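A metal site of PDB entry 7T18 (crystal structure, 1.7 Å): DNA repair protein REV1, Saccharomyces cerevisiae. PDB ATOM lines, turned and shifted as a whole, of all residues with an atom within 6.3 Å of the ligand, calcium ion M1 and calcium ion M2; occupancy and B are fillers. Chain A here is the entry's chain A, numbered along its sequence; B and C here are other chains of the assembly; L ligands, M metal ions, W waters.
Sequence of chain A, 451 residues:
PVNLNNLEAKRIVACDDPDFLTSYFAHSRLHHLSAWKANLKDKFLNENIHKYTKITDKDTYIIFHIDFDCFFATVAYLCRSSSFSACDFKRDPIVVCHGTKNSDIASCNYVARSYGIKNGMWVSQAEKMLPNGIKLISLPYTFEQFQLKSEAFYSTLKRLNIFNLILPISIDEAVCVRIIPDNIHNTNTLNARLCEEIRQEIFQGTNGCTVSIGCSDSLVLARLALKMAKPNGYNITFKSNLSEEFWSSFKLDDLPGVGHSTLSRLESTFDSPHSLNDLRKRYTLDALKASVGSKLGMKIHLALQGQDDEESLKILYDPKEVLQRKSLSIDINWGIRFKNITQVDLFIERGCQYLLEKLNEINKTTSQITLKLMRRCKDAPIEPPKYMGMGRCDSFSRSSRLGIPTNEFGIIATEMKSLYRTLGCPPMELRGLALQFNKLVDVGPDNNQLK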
ATOM      1  N   ARG A  29     -18.801  25.665  16.102  1.00  0.00           N
ATOM      2  CA  ARG A  29     -19.787  25.353  15.068  1.00  0.00           C
ATOM      3  C   ARG A  29     -19.390  25.951  13.726  1.00  0.00           C
ATOM      4  O   ARG A  29     -19.584  25.323  12.677  1.00  0.00           O
ATOM      5  CB  ARG A  29     -21.177  25.850  15.475  1.00  0.00           C
ATOM      6  CG  ARG A  29     -21.344  27.382  15.437  1.00  0.00           C
ATOM      7  CD  ARG A  29     -22.608  27.782  16.145  1.00  0.00           C
ATOM      8  NE  ARG A  29     -23.192  29.009  15.625  1.00  0.00           N
ATOM      9  CZ  ARG A  29     -22.869  30.229  16.039  1.00  0.00           C
ATOM     10  NH1 ARG A  29     -21.937  30.373  16.968  1.00  0.00           N
ATOM     11  NH2 ARG A  29     -23.473  31.297  15.524  1.00  0.00           N
ATOM     12  N   LEU A  30     -18.831  27.160  13.733  1.00  0.00           N
ATOM     13  CA  LEU A  30     -18.518  27.813  12.470  1.00  0.00           C
ATOM     14  C   LEU A  30     -17.340  27.132  11.784  1.00  0.00           C
ATOM     15  O   LEU A  30     -17.295  27.039  10.552  1.00  0.00           O
ATOM     16  CB  LEU A  30     -18.281  29.300  12.686  1.00  0.00           C
ATOM     17  CG  LEU A  30     -19.540  30.088  13.112  1.00  0.00           C
ATOM     18  CD1 LEU A  30     -19.196  31.506  13.539  1.00  0.00           C
ATOM     19  CD2 LEU A  30     -20.535  30.112  12.000  1.00  0.00           C
ATOM     20  N   LEU A  33     -18.940  24.143  10.168  1.00  0.00           N
ATOM     21  CA  LEU A  33     -19.732  24.614   8.994  1.00  0.00           C
ATOM     22  C   LEU A  33     -18.823  24.733   7.764  1.00  0.00           C
ATOM     23  O   LEU A  33     -19.202  24.225   6.698  1.00  0.00           O
ATOM     24  CB  LEU A  33     -20.377  25.958   9.335  1.00  0.00           C
ATOM     25  CG  LEU A  33     -21.893  26.021   9.178  1.00  0.00           C
ATOM     26  CD1 LEU A  33     -22.360  27.457   8.957  1.00  0.00           C
ATOM     27  CD2 LEU A  33     -22.359  25.134   8.021  1.00  0.00           C
ATOM     28  N   TRP A  36     -17.071  21.090   6.863  1.00  0.00           N
ATOM     29  CA  TRP A  36     -18.045  20.258   6.181  1.00  0.00           C
ATOM     30  C   TRP A  36     -18.242  20.681   4.735  1.00  0.00           C
ATOM     31  O   TRP A  36     -18.287  19.841   3.834  1.00  0.00           O
ATOM     32  CB  TRP A  36     -19.383  20.334   6.904  1.00  0.00           C
ATOM     33  CG  TRP A  36     -19.423  19.671   8.210  1.00  0.00           C
ATOM     34  CD1 TRP A  36     -18.750  18.551   8.602  1.00  0.00           C
ATOM     35  CD2 TRP A  36     -20.221  20.068   9.326  1.00  0.00           C
ATOM     36  NE1 TRP A  36     -19.080  18.233   9.899  1.00  0.00           N
ATOM     37  CE2 TRP A  36     -19.991  19.152  10.357  1.00  0.00           C
ATOM     38  CE3 TRP A  36     -21.140  21.113   9.540  1.00  0.00           C
ATOM     39  CZ2 TRP A  36     -20.625  19.248  11.595  1.00  0.00           C
ATOM     40  CZ3 TRP A  36     -21.764  21.206  10.757  1.00  0.00           C
ATOM     41  CH2 TRP A  36     -21.497  20.283  11.773  1.00  0.00           C
ATOM     42  N   ASP A  67     -33.551  21.642   2.227  1.00  0.00           N
ATOM     43  CA  ASP A  67     -32.818  22.113   3.395  1.00  0.00           C
ATOM     44  C   ASP A  67     -33.471  21.566   4.664  1.00  0.00           C
ATOM     45  O   ASP A  67     -34.702  21.576   4.782  1.00  0.00           O
ATOM     46  CB  ASP A  67     -32.781  23.654   3.403  1.00  0.00           C
ATOM     47  CG  ASP A  67     -32.256  24.230   4.703  1.00  0.00           C
ATOM     48  OD1 ASP A  67     -33.068  24.487   5.602  1.00  0.00           O
ATOM     49  OD2 ASP A  67     -31.031  24.409   4.819  1.00  0.00           O
ATOM     50  N   PHE A  68     -32.656  21.065   5.598  1.00  0.00           N
ATOM     51  CA  PHE A  68     -33.174  20.590   6.884  1.00  0.00           C
ATOM     52  C   PHE A  68     -33.790  21.746   7.677  1.00  0.00           C
ATOM     53  O   PHE A  68     -33.185  22.815   7.808  1.00  0.00           O
ATOM     54  CB  PHE A  68     -32.041  20.019   7.753  1.00  0.00           C
ATOM     55  CG  PHE A  68     -31.592  18.615   7.429  1.00  0.00           C
ATOM     56  CD1 PHE A  68     -30.803  18.353   6.329  1.00  0.00           C
ATOM     57  CD2 PHE A  68     -31.857  17.582   8.313  1.00  0.00           C
ATOM     58  CE1 PHE A  68     -30.313  17.070   6.068  1.00  0.00           C
ATOM     59  CE2 PHE A  68     -31.373  16.294   8.081  1.00  0.00           C
ATOM     60  CZ  PHE A  68     -30.615  16.032   6.955  1.00  0.00           C
ATOM     61  N   ASP A  69     -34.939  21.494   8.272  1.00  0.00           N
ATOM     62  CA  ASP A  69     -35.519  22.462   9.219  1.00  0.00           C
ATOM     63  C   ASP A  69     -34.706  22.404  10.521  1.00  0.00           C
ATOM     64  O   ASP A  69     -34.516  21.333  11.008  1.00  0.00           O
ATOM     65  CB  ASP A  69     -36.979  22.112   9.546  1.00  0.00           C
ATOM     66  CG  ASP A  69     -37.822  22.023   8.292  1.00  0.00           C
ATOM     67  OD1 ASP A  69     -37.700  22.906   7.488  1.00  0.00           O
ATOM     68  OD2 ASP A  69     -38.528  21.079   8.159  1.00  0.00           O
ATOM     69  N   CYS A  70     -34.441  23.566  11.090  1.00  0.00           N
ATOM     70  CA  CYS A  70     -33.632  23.810  12.308  1.00  0.00           C
ATOM     71  C   CYS A  70     -32.636  22.671  12.532  1.00  0.00           C
ATOM     72  O   CYS A  70     -32.763  21.984  13.478  1.00  0.00           O
ATOM     73  CB  CYS A  70     -34.508  24.084  13.520  1.00  0.00           C
ATOM     74  SG  CYS A  70     -35.854  22.885  13.736  1.00  0.00           S
ATOM     75  N   PHE A  71     -31.682  22.547  11.601  1.00  0.00           N
ATOM     76  CA  PHE A  71     -30.857  21.348  11.568  1.00  0.00           C
ATOM     77  C   PHE A  71     -30.249  20.922  12.906  1.00  0.00           C
ATOM     78  O   PHE A  71     -30.493  19.815  13.386  1.00  0.00           O
ATOM     79  CB  PHE A  71     -29.757  21.561  10.533  1.00  0.00           C
ATOM     80  CG  PHE A  71     -28.869  20.386  10.329  1.00  0.00           C
ATOM     81  CD1 PHE A  71     -29.398  19.140  10.082  1.00  0.00           C
ATOM     82  CD2 PHE A  71     -27.483  20.532  10.403  1.00  0.00           C
ATOM     83  CE1 PHE A  71     -28.580  18.049   9.883  1.00  0.00           C
ATOM     84  CE2 PHE A  71     -26.654  19.435  10.226  1.00  0.00           C
ATOM     85  CZ  PHE A  71     -27.200  18.203   9.958  1.00  0.00           C
ATOM     86  N   PHE A  72     -29.422  21.779  13.527  1.00  0.00           N
ATOM     87  CA  PHE A  72     -28.771  21.356  14.770  1.00  0.00           C
ATOM     88  C   PHE A  72     -29.800  21.068  15.853  1.00  0.00           C
ATOM     89  O   PHE A  72     -29.610  20.145  16.659  1.00  0.00           O
ATOM     90  CB  PHE A  72     -27.806  22.413  15.289  1.00  0.00           C
ATOM     91  CG  PHE A  72     -26.475  22.485  14.585  1.00  0.00           C
ATOM     92  CD1 PHE A  72     -26.237  21.889  13.356  1.00  0.00           C
ATOM     93  CD2 PHE A  72     -25.439  23.205  15.192  1.00  0.00           C
ATOM     94  CE1 PHE A  72     -24.999  22.008  12.739  1.00  0.00           C
ATOM     95  CE2 PHE A  72     -24.189  23.321  14.586  1.00  0.00           C
ATOM     96  CZ  PHE A  72     -23.983  22.738  13.345  1.00  0.00           C
ATOM     97  N   ALA A  73     -30.865  21.869  15.942  1.00  0.00           N
ATOM     98  CA  ALA A  73     -31.857  21.627  16.999  1.00  0.00           C
ATOM     99  C   ALA A  73     -32.566  20.294  16.787  1.00  0.00           C
ATOM    100  O   ALA A  73     -32.766  19.546  17.740  1.00  0.00           O
ATOM    101  CB  ALA A  73     -32.865  22.777  17.064  1.00  0.00           C
ATOM    102  N   ALA A 106     -26.954  28.252  18.205  1.00  0.00           N
ATOM    103  CA  ALA A 106     -26.611  27.709  16.891  1.00  0.00           C
ATOM    104  C   ALA A 106     -27.858  27.414  16.076  1.00  0.00           C
ATOM    105  O   ALA A 106     -27.880  27.643  14.858  1.00  0.00           O
ATOM    106  CB  ALA A 106     -25.758  26.455  17.069  1.00  0.00           C
ATOM    107  N   SER A 107     -28.894  26.901  16.730  1.00  0.00           N
ATOM    108  CA  SER A 107     -30.150  26.547  16.088  1.00  0.00           C
ATOM    109  C   SER A 107     -31.224  26.588  17.147  1.00  0.00           C
ATOM    110  O   SER A 107     -30.984  26.245  18.307  1.00  0.00           O
ATOM    111  CB  SER A 107     -30.068  25.144  15.466  1.00  0.00           C
ATOM    112  OG  SER A 107     -31.220  24.833  14.684  1.00  0.00           O
ATOM    113  N   CYS A 108     -32.412  27.018  16.747  1.00  0.00           N
ATOM    114  CA  CYS A 108     -33.548  26.952  17.651  1.00  0.00           C
ATOM    115  C   CYS A 108     -34.718  26.367  16.873  1.00  0.00           C
ATOM    116  O   CYS A 108     -34.817  26.556  15.664  1.00  0.00           O
ATOM    117  CB  CYS A 108     -33.919  28.328  18.209  1.00  0.00           C
ATOM    118  SG  CYS A 108     -34.206  29.565  16.923  1.00  0.00           S
ATOM    119  N   TYR A 110     -38.853  25.651  15.978  1.00  0.00           N
ATOM    120  CA  TYR A 110     -39.846  26.624  15.544  1.00  0.00           C
ATOM    121  C   TYR A 110     -40.773  27.044  16.674  1.00  0.00           C
ATOM    122  O   TYR A 110     -41.401  28.103  16.577  1.00  0.00           O
ATOM    123  CB  TYR A 110     -40.610  26.065  14.322  1.00  0.00           C
ATOM    124  CG  TYR A 110     -39.795  26.278  13.064  1.00  0.00           C
ATOM    125  CD1 TYR A 110     -38.695  25.479  12.785  1.00  0.00           C
ATOM    126  CD2 TYR A 110     -40.091  27.299  12.177  1.00  0.00           C
ATOM    127  CE1 TYR A 110     -37.910  25.697  11.647  1.00  0.00           C
ATOM    128  CE2 TYR A 110     -39.326  27.515  11.025  1.00  0.00           C
ATOM    129  CZ  TYR A 110     -38.238  26.717  10.776  1.00  0.00           C
ATOM    130  OH  TYR A 110     -37.464  26.925   9.654  1.00  0.00           O
ATOM    131  N   ARG A 113     -38.885  29.934  17.863  1.00  0.00           N
ATOM    132  CA  ARG A 113     -39.020  31.017  16.902  1.00  0.00           C
ATOM    133  C   ARG A 113     -40.370  31.698  16.981  1.00  0.00           C
ATOM    134  O   ARG A 113     -40.486  32.864  16.598  1.00  0.00           O
ATOM    135  CB  ARG A 113     -38.775  30.491  15.482  1.00  0.00           C
ATOM    136  CG  ARG A 113     -37.352  29.969  15.272  1.00  0.00           C
ATOM    137  CD  ARG A 113     -37.118  29.420  13.866  1.00  0.00           C
ATOM    138  NE  ARG A 113     -35.879  28.643  13.832  1.00  0.00           N
ATOM    139  CZ  ARG A 113     -35.161  28.398  12.744  1.00  0.00           C
ATOM    140  NH1 ARG A 113     -35.556  28.874  11.566  1.00  0.00           N
ATOM    141  NH2 ARG A 113     -34.040  27.684  12.838  1.00  0.00           N
ATOM    142  N   ASN A 119     -31.775  32.047  15.266  1.00  0.00           N
ATOM    143  CA  ASN A 119     -30.402  31.564  15.232  1.00  0.00           C
ATOM    144  C   ASN A 119     -29.448  32.741  15.370  1.00  0.00           C
ATOM    145  O   ASN A 119     -29.652  33.808  14.777  1.00  0.00           O
ATOM    146  CB  ASN A 119     -30.108  30.838  13.914  1.00  0.00           C
ATOM    147  CG  ASN A 119     -30.804  29.496  13.805  1.00  0.00           C
ATOM    148  OD1 ASN A 119     -31.531  29.094  14.699  1.00  0.00           O
ATOM    149  ND2 ASN A 119     -30.572  28.797  12.689  1.00  0.00           N
ATOM    150  N   TYR A 141     -24.300  20.458  21.628  1.00  0.00           N
ATOM    151  CA  TYR A 141     -23.973  20.049  20.276  1.00  0.00           C
ATOM    152  C   TYR A 141     -23.699  18.549  20.194  1.00  0.00           C
ATOM    153  O   TYR A 141     -23.169  17.929  21.118  1.00  0.00           O
ATOM    154  CB  TYR A 141     -22.734  20.787  19.784  1.00  0.00           C
ATOM    155  CG  TYR A 141     -22.862  22.277  19.651  1.00  0.00           C
ATOM    156  CD1 TYR A 141     -22.629  23.119  20.739  1.00  0.00           C
ATOM    157  CD2 TYR A 141     -23.189  22.865  18.434  1.00  0.00           C
ATOM    158  CE1 TYR A 141     -22.722  24.495  20.619  1.00  0.00           C
ATOM    159  CE2 TYR A 141     -23.281  24.243  18.304  1.00  0.00           C
ATOM    160  CZ  TYR A 141     -23.029  25.048  19.388  1.00  0.00           C
ATOM    161  OH  TYR A 141     -23.118  26.430  19.239  1.00  0.00           O
ATOM    162  N   ILE A 169     -24.707  22.555  -0.986  1.00  0.00           N
ATOM    163  CA  ILE A 169     -24.644  23.919  -0.503  1.00  0.00           C
ATOM    164  C   ILE A 169     -24.032  23.974   0.892  1.00  0.00           C
ATOM    165  O   ILE A 169     -23.208  24.837   1.183  1.00  0.00           O
ATOM    166  CB  ILE A 169     -26.044  24.563  -0.502  1.00  0.00           C
ATOM    167  CG1 ILE A 169     -26.631  24.581  -1.909  1.00  0.00           C
ATOM    168  CG2 ILE A 169     -25.993  25.962   0.090  1.00  0.00           C
ATOM    169  CD1 ILE A 169     -25.853  25.473  -2.870  1.00  0.00           C
ATOM    170  N   SER A 170     -24.434  23.037   1.752  1.00  0.00           N
ATOM    171  CA  SER A 170     -23.922  22.999   3.111  1.00  0.00           C
ATOM    172  C   SER A 170     -24.219  21.620   3.693  1.00  0.00           C
ATOM    173  O   SER A 170     -24.731  20.730   3.003  1.00  0.00           O
ATOM    174  CB  SER A 170     -24.552  24.100   3.963  1.00  0.00           C
ATOM    175  OG  SER A 170     -25.781  23.657   4.465  1.00  0.00           O
ATOM    176  N   ILE A 171     -23.859  21.448   4.958  1.00  0.00           N
ATOM    177  CA  ILE A 171     -24.082  20.200   5.681  1.00  0.00           C
ATOM    178  C   ILE A 171     -25.548  19.767   5.587  1.00  0.00           C
ATOM    179  O   ILE A 171     -25.850  18.567   5.543  1.00  0.00           O
ATOM    180  CB  ILE A 171     -23.619  20.375   7.148  1.00  0.00           C
ATOM    181  CG1 ILE A 171     -23.728  19.049   7.916  1.00  0.00           C
ATOM    182  CG2 ILE A 171     -24.427  21.466   7.876  1.00  0.00           C
ATOM    183  CD1 ILE A 171     -22.590  18.113   7.616  1.00  0.00           C
ATOM    184  N   ASP A 172     -26.474  20.732   5.536  1.00  0.00           N
ATOM    185  CA  ASP A 172     -27.899  20.414   5.596  1.00  0.00           C
ATOM    186  C   ASP A 172     -28.688  20.928   4.390  1.00  0.00           C
ATOM    187  O   ASP A 172     -29.915  21.048   4.469  1.00  0.00           O
ATOM    188  CB  ASP A 172     -28.519  20.961   6.896  1.00  0.00           C
ATOM    189  CG  ASP A 172     -28.843  22.443   6.811  1.00  0.00           C
ATOM    190  OD1 ASP A 172     -28.091  23.176   6.154  1.00  0.00           O
ATOM    191  OD2 ASP A 172     -29.855  22.879   7.393  1.00  0.00           O
ATOM    192  N   GLU A 173     -28.027  21.212   3.266  1.00  0.00           N
ATOM    193  CA  GLU A 173     -28.730  21.919   2.206  1.00  0.00           C
ATOM    194  C   GLU A 173     -28.117  21.564   0.862  1.00  0.00           C
ATOM    195  O   GLU A 173     -26.890  21.566   0.725  1.00  0.00           O
ATOM    196  CB  GLU A 173     -28.665  23.431   2.441  1.00  0.00           C
ATOM    197  CG  GLU A 173     -29.403  24.275   1.434  1.00  0.00           C
ATOM    198  CD  GLU A 173     -29.293  25.751   1.782  1.00  0.00           C
ATOM    199  OE1 GLU A 173     -29.674  26.607   0.952  1.00  0.00           O
ATOM    200  OE2 GLU A 173     -28.824  26.044   2.902  1.00  0.00           O
ATOM    201  N   LYS A 230     -41.096  26.639   4.733  1.00  0.00           N
ATOM    202  CA  LYS A 230     -40.718  26.216   6.075  1.00  0.00           C
ATOM    203  C   LYS A 230     -41.806  26.535   7.095  1.00  0.00           C
ATOM    204  O   LYS A 230     -42.528  27.532   6.950  1.00  0.00           O
ATOM    205  CB  LYS A 230     -39.413  26.911   6.495  1.00  0.00           C
ATOM    206  CG  LYS A 230     -38.181  26.298   5.842  1.00  0.00           C
ATOM    207  CD  LYS A 230     -36.918  27.068   6.166  1.00  0.00           C
ATOM    208  CE  LYS A 230     -35.680  26.231   5.841  1.00  0.00           C
ATOM    209  NZ  LYS A 230     -35.671  24.891   6.532  1.00  0.00           N
ATOM    210  P    DG B  12     -25.705  30.059   0.502  1.00  0.00           P
ATOM    211  OP1  DG B  12     -25.319  29.488  -0.831  1.00  0.00           O
ATOM    212  OP2  DG B  12     -27.058  30.508   0.719  1.00  0.00           O
ATOM    213  O5'  DG B  12     -25.417  28.952   1.587  1.00  0.00           O
ATOM    214  C5'  DG B  12     -26.272  28.716   2.699  1.00  0.00           C
ATOM    215  C4'  DG B  12     -25.410  28.064   3.744  1.00  0.00           C
ATOM    216  O4'  DG B  12     -24.290  28.945   3.944  1.00  0.00           O
ATOM    217  C3'  DG B  12     -26.013  27.852   5.121  1.00  0.00           C
ATOM    218  O3'  DG B  12     -26.613  26.563   5.236  1.00  0.00           O
ATOM    219  C2'  DG B  12     -24.795  27.923   6.010  1.00  0.00           C
ATOM    220  C1'  DG B  12     -23.769  28.726   5.196  1.00  0.00           C
ATOM    221  N9   DG B  12     -23.459  30.013   5.808  1.00  0.00           N
ATOM    222  C8   DG B  12     -24.327  30.982   6.252  1.00  0.00           C
ATOM    223  N7   DG B  12     -23.739  31.910   6.941  1.00  0.00           N
ATOM    224  C5   DG B  12     -22.427  31.486   7.032  1.00  0.00           C
ATOM    225  C6   DG B  12     -21.321  32.065   7.695  1.00  0.00           C
ATOM    226  O6   DG B  12     -21.262  33.117   8.311  1.00  0.00           O
ATOM    227  N1   DG B  12     -20.157  31.313   7.509  1.00  0.00           N
ATOM    228  C2   DG B  12     -20.101  30.126   6.834  1.00  0.00           C
ATOM    229  N2   DG B  12     -18.921  29.521   6.804  1.00  0.00           N
ATOM    230  N3   DG B  12     -21.125  29.573   6.221  1.00  0.00           N
ATOM    231  C4   DG B  12     -22.242  30.316   6.330  1.00  0.00           C
ATOM    232  P    DC C   5     -13.914  32.971  14.394  1.00  0.00           P
ATOM    233  OP1  DC C   5     -13.005  32.717  15.527  1.00  0.00           O
ATOM    234  OP2  DC C   5     -13.724  34.185  13.575  1.00  0.00           O
ATOM    235  O5'  DC C   5     -13.908  31.766  13.355  1.00  0.00           O
ATOM    236  C5'  DC C   5     -14.045  30.436  13.817  1.00  0.00           C
ATOM    237  C4'  DC C   5     -14.154  29.468  12.663  1.00  0.00           C
ATOM    238  O4'  DC C   5     -15.394  29.680  11.951  1.00  0.00           O
ATOM    239  C3'  DC C   5     -13.069  29.593  11.607  1.00  0.00           C
ATOM    240  O3'  DC C   5     -12.866  28.324  11.053  1.00  0.00           O
ATOM    241  C2'  DC C   5     -13.683  30.554  10.583  1.00  0.00           C
ATOM    242  C1'  DC C   5     -15.145  30.141  10.628  1.00  0.00           C
ATOM    243  N1   DC C   5     -16.121  31.233  10.377  1.00  0.00           N
ATOM    244  C2   DC C   5     -17.063  31.087   9.364  1.00  0.00           C
ATOM    245  O2   DC C   5     -17.026  30.068   8.657  1.00  0.00           O
ATOM    246  N3   DC C   5     -17.995  32.041   9.195  1.00  0.00           N
ATOM    247  C4   DC C   5     -18.001  33.107   9.978  1.00  0.00           C
ATOM    248  N4   DC C   5     -18.932  34.026   9.772  1.00  0.00           N
ATOM    249  C5   DC C   5     -17.056  33.279  11.039  1.00  0.00           C
ATOM    250  C6   DC C   5     -16.153  32.314  11.200  1.00  0.00           C
HETATM  251  P1  LIG L   1     -29.394  27.082   8.589  1.00  0.00           P
HETATM  252  O1  LIG L   1     -29.949  26.271   7.516  1.00  0.00           O
HETATM  253  O2  LIG L   1     -29.160  28.484   8.261  1.00  0.00           O
HETATM  254  O3  LIG L   1     -30.366  27.077   9.853  1.00  0.00           O
HETATM  255  P2  LIG L   1     -31.346  26.010  10.528  1.00  0.00           P
HETATM  256  O4  LIG L   1     -31.320  24.820   9.713  1.00  0.00           O
HETATM  257  O5  LIG L   1     -30.982  25.853  12.025  1.00  0.00           O
HETATM  258  O6  LIG L   1     -32.792  26.661  10.450  1.00  0.00           O
HETATM  259  P3  LIG L   1     -33.775  26.808   9.200  1.00  0.00           P
HETATM  260  O7  LIG L   1     -33.007  26.352   7.995  1.00  0.00           O
HETATM  261  O8  LIG L   1     -35.012  25.918   9.455  1.00  0.00           O
HETATM  262  O9  LIG L   1     -34.190  28.290   9.152  1.00  0.00           O
HETATM  263  O10 LIG L   1     -28.044  26.441   9.098  1.00  0.00           O
HETATM  264  C1  LIG L   1     -27.871  25.026   9.233  1.00  0.00           C
HETATM  265  C2  LIG L   1     -27.139  24.732  10.515  1.00  0.00           C
HETATM  266  O11 LIG L   1     -25.825  25.300  10.414  1.00  0.00           O
HETATM  267  C3  LIG L   1     -27.762  25.373  11.750  1.00  0.00           C
HETATM  268  O12 LIG L   1     -28.698  24.501  12.379  1.00  0.00           O
HETATM  269  C4  LIG L   1     -26.577  25.665  12.637  1.00  0.00           C
HETATM  270  C5  LIG L   1     -25.429  25.862  11.659  1.00  0.00           C
HETATM  271  N1  LIG L   1     -25.109  27.276  11.440  1.00  0.00           N
HETATM  272  C6  LIG L   1     -24.202  27.884  12.314  1.00  0.00           C
HETATM  273  O13 LIG L   1     -23.700  27.241  13.218  1.00  0.00           O
HETATM  274  N2  LIG L   1     -23.874  29.225  12.133  1.00  0.00           N
HETATM  275  C7  LIG L   1     -24.509  29.854  11.142  1.00  0.00           C
HETATM  276  O14 LIG L   1     -24.221  31.040  11.016  1.00  0.00           O
HETATM  277  C8  LIG L   1     -25.440  29.306  10.235  1.00  0.00           C
HETATM  278  C9  LIG L   1     -26.090  30.099   9.129  1.00  0.00           C
HETATM  279  C10 LIG L   1     -25.802  27.965  10.399  1.00  0.00           C
HETATM  280 CA    CA M   1     -31.587  24.497   7.412  1.00  0.00          CA
HETATM  281 CA    CA M   2     -28.775  25.390   5.403  1.00  0.00          CA
HETATM  282  O   HOH W   1     -26.550  32.345  12.847  1.00  0.00           O
HETATM  283  O   HOH W   2     -32.553  30.430  10.044  1.00  0.00           O
HETATM  284  O   HOH W   3     -29.370  30.125  10.419  1.00  0.00           O
HETATM  285  O   HOH W   4     -35.286  29.798   7.156  1.00  0.00           O
HETATM  286  O   HOH W   5     -22.973  33.814  10.369  1.00  0.00           O
HETATM  287  O   HOH W   6     -25.795  29.263  14.230  1.00  0.00           O
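Calcium ion M2 is bound by the side-chain carboxylate (OD1) of Asp 172 (2.4 Å), O3' of DG 12 of chain B (2.5 Å), the side-chain carboxylate (OD2) of Asp 67 (2.5 Å), an oxygen (O1) of the ligand (2.6 Å) and the side-chain carboxylate (OE2) of Glu 173 (2.6 Å).
Calcium ion M2 has five donor atoms within binding distance.
Calcium ion M1 is bound by the side-chain carboxylate (OD1) of Asp 67.
An oxygen (O4) of the ligand binds calcium ion M1 (2.3 Å).
Calcium ion M1 is bound by O of Phe 68 (2.4 Å).
OD2 of Asp 172 is bound to calcium ion M1 (2.4 Å).
Calcium ion M1 is bound by O7 of the ligand (2.4 Å).
Calcium ion M1 is bound by an oxygen (O1) of the ligand (2.4 Å).
The side-chain carboxylate (OD2) of Asp 67 is bound to calcium ion M1 (2.7 Å).
Calcium ion M1 has seven donor atoms within binding distance.
Leu 30 touches the ligand.
Leu 33 touches the ligand.
Asp 69 touches the ligand.
Ala 106 touches the ligand (O to C4, 3.2 Å).
Hydrophobic or aromatic side chains that line the ligand: Leu 30, Leu 33, Phe 71, Phe 72 and Tyr 110.
17 residues have an atom within 4 Å of the ligand: Arg 29, Leu 30, Leu 33, Asp 67, Phe 68, Asp 69, Cys 70, Phe 71, Phe 72, Ala 106, Ser 107, Tyr 110, Arg 113, Asn 119, Asp 172, Lys 230 and DG 12 of chain B.
Merely in contact with calcium ion M2: Ser 170 (3.6 Å).
Within 4 Å of calcium ion M2: Asp 67, Ser 170, Asp 172, Glu 173 and DG 12 of chain B.
The side-chain hydroxyl (OG) of Ser 107 sits close to the backbone carbonyl oxygen (O) of Cys 70, 3.5 Å away.
O2 of DC 5 of chain C sits close to N2 of DG 12 of chain B, 2.7 Å away.
NZ of Lys 230 lies close to OD1 of Asp 67 (2.8 Å).
The side-chain amino group (NZ) of Lys 230 is in salt-bridge range of the side-chain carboxylate (OD1) of Asp 69 (3.0 Å).
NE of Arg 113 is in hydrogen-bond range of O of Cys 108, at 3.0 Å.
NH2 of Arg 113 is in hydrogen-bond range of OD1 of Asn 119 (3.4 Å).
O3' of DG 12 of chain B lies close to the side-chain hydroxyl (OG) of Ser 170 (3.1 Å).
The side-chain amino group (NZ) of Lys 230 sits close to the backbone carbonyl oxygen (O) of Phe 68, at 3.5 Å.
Of the 26 residues printed, 3 come within 4 Å of calcium ion M1.
The nearest printed residue that does not touch calcium ion M1 is Lys 230 (4.2 Å).
Water W3 bridges O2 of the ligand (2.7 Å) and ND2 of Asn 119 (2.9 Å).
Water W6 lies within hydrogen-bond range of O of Ala 106, N2 of the ligand and NE of Arg 29.
Water W5 lies within hydrogen-bond range of O6 of DG 12 of chain B (2.8 Å) and O14 of the ligand (3.1 Å).
The side-chain amino group of Lys 230 is in salt-bridge range of an oxygen (O8) of the ligand (3.2 Å).
An oxygen (O13) of the ligand is in hydrogen-bond range of the guanidinium group of Arg 29 (3.0 Å).
ND2 of Asn 119 is in hydrogen-bond range of O5 of the ligand (3.0 Å).
An oxygen (O8) of the ligand is in hydrogen-bond range of the side-chain hydroxyl (OH) of Tyr 110 (2.7 Å).
An oxygen (O5) of the ligand lies within hydrogen-bond range of the side-chain hydroxyl (OG) of Ser 107 (2.9 Å).
The backbone NH of Phe 71 sits at hydrogen-bond distance from an oxygen (O5) of the ligand (3.4 Å).
N of Phe 72 sits at hydrogen-bond distance from O12 of the ligand, at 3.0 Å.
The guanidinium group of Arg 113 is in salt-bridge range of an oxygen (O9) of the ligand (2.8 Å).
The backbone NH of Cys 70 lies within hydrogen-bond range of an oxygen (O8) of the ligand (2.9 Å).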
